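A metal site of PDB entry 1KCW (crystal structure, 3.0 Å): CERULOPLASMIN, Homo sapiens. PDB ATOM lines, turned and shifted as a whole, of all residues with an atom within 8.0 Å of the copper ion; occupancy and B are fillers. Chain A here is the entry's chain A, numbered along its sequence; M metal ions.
The backbone carbonyl oxygen (O) of Val 275 sits at hydrogen-bond distance from the side-chain amide nitrogen (ND2) of Asn 321 (2.8 Å). N of Asn 321 sits close to SG of Cys 319 (3.8 Å). A ring nitrogen (NE2) of His 324 sits close to the side-chain amide nitrogen of Asn 321, 3.3 Å away. The backbone carbonyl oxygen of His 324 lies within hydrogen-bond range of the backbone NH of Leu 329, 3.4 Å away. The backbone NH (N) of Ala 277 lies close to the side-chain sulfur (SG) of Cys 319 (3.4 Å). The side-chain carboxylate (OD2) of Asp 274 sits at hydrogen-bond distance from a ring nitrogen (NE2) of His 276. A ring nitrogen (NE2) of His 324 is in hydrogen-bond range of the backbone carbonyl oxygen of Val 273 (3.1 Å). The backbone NH (N) of His 276 lies within hydrogen-bond range of the backbone carbonyl oxygen (O) of Leu 297 (3.0 Å).
Residues that only touch the copper ion: Val 275 (3.7 Å) and Leu 329 (3.7 Å). Along chain A the residues within 4 Å of the copper ion span positions 275 to 329. The nearest printed residue that does not touch the copper ion is Asn 321 (4.01 Å).
The copper ion is bound by SG of Cys 319 (2.0 Å), ND1 of His 324 (2.1 Å) and ND1 of His 276 (2.1 Å). The copper ion has three donor atoms within binding distance.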
ATOM      1  N   PHE A 202      26.664  11.647  16.885  1.00  0.00           N
ATOM      2  CA  PHE A 202      26.194  12.719  17.752  1.00  0.00           C
ATOM      3  C   PHE A 202      26.724  12.334  19.108  1.00  0.00           C
ATOM      4  O   PHE A 202      26.743  11.145  19.426  1.00  0.00           O
ATOM      5  CB  PHE A 202      24.668  12.810  17.788  1.00  0.00           C
ATOM      6  CG  PHE A 202      24.075  13.561  16.625  1.00  0.00           C
ATOM      7  CD1 PHE A 202      24.233  13.102  15.328  1.00  0.00           C
ATOM      8  CD2 PHE A 202      23.398  14.746  16.842  1.00  0.00           C
ATOM      9  CE1 PHE A 202      23.728  13.799  14.274  1.00  0.00           C
ATOM     10  CE2 PHE A 202      22.877  15.460  15.781  1.00  0.00           C
ATOM     11  CZ  PHE A 202      23.041  14.987  14.492  1.00  0.00           C
ATOM     12  N   SER A 203      27.216  13.332  19.846  1.00  0.00           N
ATOM     13  CA  SER A 203      27.749  13.120  21.190  1.00  0.00           C
ATOM     14  C   SER A 203      28.113  14.430  21.908  1.00  0.00           C
ATOM     15  O   SER A 203      28.603  15.373  21.289  1.00  0.00           O
ATOM     16  CB  SER A 203      28.986  12.217  21.138  1.00  0.00           C
ATOM     17  OG  SER A 203      29.678  12.220  22.373  1.00  0.00           O
ATOM     18  N   VAL A 204      27.831  14.463  23.208  1.00  0.00           N
ATOM     19  CA  VAL A 204      28.283  15.542  24.088  1.00  0.00           C
ATOM     20  C   VAL A 204      29.629  15.070  24.587  1.00  0.00           C
ATOM     21  O   VAL A 204      29.736  14.623  25.743  1.00  0.00           O
ATOM     22  CB  VAL A 204      27.320  15.683  25.292  1.00  0.00           C
ATOM     23  CG1 VAL A 204      27.770  16.803  26.206  1.00  0.00           C
ATOM     24  CG2 VAL A 204      25.892  15.883  24.820  1.00  0.00           C
ATOM     25  N   TYR A 241      29.164  19.659  23.010  1.00  0.00           N
ATOM     26  CA  TYR A 241      28.031  19.217  22.200  1.00  0.00           C
ATOM     27  C   TYR A 241      28.443  19.252  20.747  1.00  0.00           C
ATOM     28  O   TYR A 241      28.568  20.327  20.176  1.00  0.00           O
ATOM     29  CB  TYR A 241      26.849  20.145  22.483  1.00  0.00           C
ATOM     30  CG  TYR A 241      26.406  20.165  23.944  1.00  0.00           C
ATOM     31  CD1 TYR A 241      27.149  20.806  24.920  1.00  0.00           C
ATOM     32  CD2 TYR A 241      25.234  19.524  24.345  1.00  0.00           C
ATOM     33  CE1 TYR A 241      26.718  20.809  26.258  1.00  0.00           C
ATOM     34  CE2 TYR A 241      24.821  19.521  25.670  1.00  0.00           C
ATOM     35  CZ  TYR A 241      25.559  20.155  26.616  1.00  0.00           C
ATOM     36  OH  TYR A 241      25.124  20.130  27.921  1.00  0.00           O
ATOM     37  N   SER A 242      28.603  18.103  20.103  1.00  0.00           N
ATOM     38  CA  SER A 242      29.103  18.117  18.743  1.00  0.00           C
ATOM     39  C   SER A 242      28.789  17.009  17.952  1.00  0.00           C
ATOM     40  O   SER A 242      28.752  15.884  18.422  1.00  0.00           O
ATOM     41  CB  SER A 242      30.600  18.242  18.852  1.00  0.00           C
ATOM     42  OG  SER A 242      31.144  17.213  19.667  1.00  0.00           O
ATOM     43  N   VAL A 273      22.798  12.148  29.323  1.00  0.00           N
ATOM     44  CA  VAL A 273      22.280  13.437  28.906  1.00  0.00           C
ATOM     45  C   VAL A 273      22.420  13.369  27.409  1.00  0.00           C
ATOM     46  O   VAL A 273      22.375  14.390  26.753  1.00  0.00           O
ATOM     47  CB  VAL A 273      23.098  14.652  29.474  1.00  0.00           C
ATOM     48  CG1 VAL A 273      23.250  14.528  30.973  1.00  0.00           C
ATOM     49  CG2 VAL A 273      24.455  14.765  28.805  1.00  0.00           C
ATOM     50  N   ASP A 274      22.605  12.168  26.889  1.00  0.00           N
ATOM     51  CA  ASP A 274      22.777  12.028  25.453  1.00  0.00           C
ATOM     52  C   ASP A 274      21.525  11.562  24.729  1.00  0.00           C
ATOM     53  O   ASP A 274      21.502  10.533  24.049  1.00  0.00           O
ATOM     54  CB  ASP A 274      23.959  11.134  25.144  1.00  0.00           C
ATOM     55  CG  ASP A 274      25.249  11.892  25.130  1.00  0.00           C
ATOM     56  OD1 ASP A 274      25.907  12.020  26.190  1.00  0.00           O
ATOM     57  OD2 ASP A 274      25.602  12.365  24.049  1.00  0.00           O
ATOM     58  N   VAL A 275      20.480  12.380  24.881  1.00  0.00           N
ATOM     59  CA  VAL A 275      19.211  12.117  24.270  1.00  0.00           C
ATOM     60  C   VAL A 275      19.240  13.013  23.032  1.00  0.00           C
ATOM     61  O   VAL A 275      19.044  14.219  23.129  1.00  0.00           O
ATOM     62  CB  VAL A 275      18.130  12.540  25.239  1.00  0.00           C
ATOM     63  CG1 VAL A 275      16.778  12.398  24.616  1.00  0.00           C
ATOM     64  CG2 VAL A 275      18.226  11.712  26.487  1.00  0.00           C
ATOM     65  N   HIS A 276      19.580  12.426  21.891  1.00  0.00           N
ATOM     66  CA  HIS A 276      19.675  13.186  20.664  1.00  0.00           C
ATOM     67  C   HIS A 276      18.487  13.043  19.758  1.00  0.00           C
ATOM     68  O   HIS A 276      17.736  12.094  19.868  1.00  0.00           O
ATOM     69  CB  HIS A 276      20.943  12.803  19.879  1.00  0.00           C
ATOM     70  CG  HIS A 276      22.205  13.001  20.665  1.00  0.00           C
ATOM     71  ND1 HIS A 276      22.672  14.251  20.937  1.00  0.00           N
ATOM     72  CD2 HIS A 276      22.874  12.091  21.404  1.00  0.00           C
ATOM     73  CE1 HIS A 276      23.609  14.083  21.857  1.00  0.00           C
ATOM     74  NE2 HIS A 276      23.767  12.785  22.165  1.00  0.00           N
ATOM     75  N   ALA A 277      18.394  13.966  18.803  1.00  0.00           N
ATOM     76  CA  ALA A 277      17.321  13.999  17.817  1.00  0.00           C
ATOM     77  C   ALA A 277      17.917  14.562  16.548  1.00  0.00           C
ATOM     78  O   ALA A 277      17.770  15.745  16.267  1.00  0.00           O
ATOM     79  CB  ALA A 277      16.209  14.884  18.302  1.00  0.00           C
ATOM     80  N   ALA A 278      18.651  13.740  15.821  1.00  0.00           N
ATOM     81  CA  ALA A 278      19.278  14.179  14.587  1.00  0.00           C
ATOM     82  C   ALA A 278      18.206  14.622  13.614  1.00  0.00           C
ATOM     83  O   ALA A 278      17.227  13.918  13.412  1.00  0.00           O
ATOM     84  CB  ALA A 278      20.072  13.065  13.987  1.00  0.00           C
ATOM     85  N   LEU A 297      19.025   9.187  18.768  1.00  0.00           N
ATOM     86  CA  LEU A 297      20.258   8.467  19.017  1.00  0.00           C
ATOM     87  C   LEU A 297      20.611   8.622  20.462  1.00  0.00           C
ATOM     88  O   LEU A 297      20.505   9.713  21.015  1.00  0.00           O
ATOM     89  CB  LEU A 297      21.373   9.078  18.194  1.00  0.00           C
ATOM     90  CG  LEU A 297      21.135   8.957  16.685  1.00  0.00           C
ATOM     91  CD1 LEU A 297      22.264   9.625  15.887  1.00  0.00           C
ATOM     92  CD2 LEU A 297      21.018   7.499  16.309  1.00  0.00           C
ATOM     93  N   SER A 318      20.877  19.294  12.691  1.00  0.00           N
ATOM     94  CA  SER A 318      20.969  19.677  14.085  1.00  0.00           C
ATOM     95  C   SER A 318      20.394  18.586  14.965  1.00  0.00           C
ATOM     96  O   SER A 318      19.954  17.548  14.462  1.00  0.00           O
ATOM     97  CB  SER A 318      20.271  21.017  14.350  1.00  0.00           C
ATOM     98  OG  SER A 318      18.885  20.934  14.107  1.00  0.00           O
ATOM     99  N   CYS A 319      20.432  18.803  16.265  1.00  0.00           N
ATOM    100  CA  CYS A 319      19.888  17.837  17.176  1.00  0.00           C
ATOM    101  C   CYS A 319      18.721  18.555  17.869  1.00  0.00           C
ATOM    102  O   CYS A 319      18.931  19.407  18.741  1.00  0.00           O
ATOM    103  CB  CYS A 319      20.969  17.412  18.161  1.00  0.00           C
ATOM    104  SG  CYS A 319      20.383  16.564  19.571  1.00  0.00           S
ATOM    105  N   GLN A 320      17.500  18.224  17.460  1.00  0.00           N
ATOM    106  CA  GLN A 320      16.304  18.857  17.995  1.00  0.00           C
ATOM    107  C   GLN A 320      16.139  18.806  19.491  1.00  0.00           C
ATOM    108  O   GLN A 320      15.175  19.367  20.034  1.00  0.00           O
ATOM    109  CB  GLN A 320      15.066  18.340  17.294  1.00  0.00           C
ATOM    110  CG  GLN A 320      14.945  18.771  15.856  1.00  0.00           C
ATOM    111  CD  GLN A 320      15.403  20.200  15.684  1.00  0.00           C
ATOM    112  OE1 GLN A 320      14.941  21.086  16.400  1.00  0.00           O
ATOM    113  NE2 GLN A 320      16.279  20.631  14.796  1.00  0.00           N
ATOM    114  N   ASN A 321      17.006  18.131  20.201  1.00  0.00           N
ATOM    115  CA  ASN A 321      16.948  18.258  21.639  1.00  0.00           C
ATOM    116  C   ASN A 321      17.209  19.733  21.887  1.00  0.00           C
ATOM    117  O   ASN A 321      18.253  20.242  21.490  1.00  0.00           O
ATOM    118  CB  ASN A 321      17.976  17.350  22.295  1.00  0.00           C
ATOM    119  CG  ASN A 321      18.115  17.611  23.774  1.00  0.00           C
ATOM    120  OD1 ASN A 321      17.803  18.692  24.259  1.00  0.00           O
ATOM    121  ND2 ASN A 321      18.581  16.599  24.495  1.00  0.00           N
ATOM    122  N   LEU A 322      16.267  20.441  22.504  1.00  0.00           N
ATOM    123  CA  LEU A 322      16.454  21.873  22.722  1.00  0.00           C
ATOM    124  C   LEU A 322      17.726  22.258  23.416  1.00  0.00           C
ATOM    125  O   LEU A 322      18.494  23.041  22.864  1.00  0.00           O
ATOM    126  CB  LEU A 322      15.269  22.508  23.448  1.00  0.00           C
ATOM    127  CG  LEU A 322      13.933  22.357  22.712  1.00  0.00           C
ATOM    128  CD1 LEU A 322      12.872  22.963  23.598  1.00  0.00           C
ATOM    129  CD2 LEU A 322      13.919  22.971  21.296  1.00  0.00           C
ATOM    130  N   ASN A 323      17.989  21.682  24.589  1.00  0.00           N
ATOM    131  CA  ASN A 323      19.224  22.027  25.291  1.00  0.00           C
ATOM    132  C   ASN A 323      20.497  21.828  24.474  1.00  0.00           C
ATOM    133  O   ASN A 323      21.434  22.622  24.567  1.00  0.00           O
ATOM    134  CB  ASN A 323      19.293  21.301  26.612  1.00  0.00           C
ATOM    135  CG  ASN A 323      18.404  21.925  27.630  1.00  0.00           C
ATOM    136  OD1 ASN A 323      17.572  22.782  27.299  1.00  0.00           O
ATOM    137  ND2 ASN A 323      18.569  21.543  28.889  1.00  0.00           N
ATOM    138  N   HIS A 324      20.518  20.816  23.632  1.00  0.00           N
ATOM    139  CA  HIS A 324      21.669  20.558  22.816  1.00  0.00           C
ATOM    140  C   HIS A 324      21.716  21.598  21.723  1.00  0.00           C
ATOM    141  O   HIS A 324      22.766  22.149  21.431  1.00  0.00           O
ATOM    142  CB  HIS A 324      21.627  19.116  22.266  1.00  0.00           C
ATOM    143  CG  HIS A 324      21.787  18.061  23.324  1.00  0.00           C
ATOM    144  ND1 HIS A 324      21.772  16.728  23.035  1.00  0.00           N
ATOM    145  CD2 HIS A 324      21.820  18.223  24.679  1.00  0.00           C
ATOM    146  CE1 HIS A 324      21.782  16.094  24.178  1.00  0.00           C
ATOM    147  NE2 HIS A 324      21.802  16.966  25.214  1.00  0.00           N
ATOM    148  N   LEU A 325      20.558  21.954  21.189  1.00  0.00           N
ATOM    149  CA  LEU A 325      20.497  22.958  20.129  1.00  0.00           C
ATOM    150  C   LEU A 325      21.107  24.311  20.563  1.00  0.00           C
ATOM    151  O   LEU A 325      21.852  24.925  19.804  1.00  0.00           O
ATOM    152  CB  LEU A 325      19.053  23.161  19.708  1.00  0.00           C
ATOM    153  CG  LEU A 325      18.846  24.125  18.542  1.00  0.00           C
ATOM    154  CD1 LEU A 325      18.922  23.355  17.218  1.00  0.00           C
ATOM    155  CD2 LEU A 325      17.474  24.773  18.677  1.00  0.00           C
ATOM    156  N   LEU A 329      24.834  22.489  18.765  1.00  0.00           N
ATOM    157  CA  LEU A 329      25.074  21.211  18.133  1.00  0.00           C
ATOM    158  C   LEU A 329      24.489  21.327  16.752  1.00  0.00           C
ATOM    159  O   LEU A 329      23.519  20.652  16.421  1.00  0.00           O
ATOM    160  CB  LEU A 329      24.380  20.068  18.895  1.00  0.00           C
ATOM    161  CG  LEU A 329      25.007  18.664  18.709  1.00  0.00           C
ATOM    162  CD1 LEU A 329      24.611  17.792  19.862  1.00  0.00           C
ATOM    163  CD2 LEU A 329      24.654  18.013  17.384  1.00  0.00           C
ATOM    164  N   GLU A 633      16.243  16.778  27.171  1.00  0.00           N
ATOM    165  CA  GLU A 633      16.619  15.404  27.468  1.00  0.00           C
ATOM    166  C   GLU A 633      15.785  14.778  28.564  1.00  0.00           C
ATOM    167  O   GLU A 633      16.025  13.633  28.973  1.00  0.00           O
ATOM    168  CB  GLU A 633      18.107  15.309  27.806  1.00  0.00           C
ATOM    169  CG  GLU A 633      18.506  15.940  29.146  1.00  0.00           C
ATOM    170  CD  GLU A 633      19.030  17.361  29.009  1.00  0.00           C
ATOM    171  OE1 GLU A 633      19.379  17.806  27.884  1.00  0.00           O
ATOM    172  OE2 GLU A 633      19.104  18.038  30.062  1.00  0.00           O
ATOM    173  N   PRO A 660      12.546  13.816  22.293  1.00  0.00           N
ATOM    174  CA  PRO A 660      12.485  15.067  21.541  1.00  0.00           C
ATOM    175  C   PRO A 660      12.227  14.921  20.041  1.00  0.00           C
ATOM    176  O   PRO A 660      13.070  14.401  19.319  1.00  0.00           O
ATOM    177  CB  PRO A 660      13.849  15.665  21.808  1.00  0.00           C
ATOM    178  CG  PRO A 660      14.051  15.297  23.258  1.00  0.00           C
ATOM    179  CD  PRO A 660      13.671  13.841  23.242  1.00  0.00           C
HETATM  180 CU    CU M   1      21.579  16.038  21.112  1.00  0.00          CU
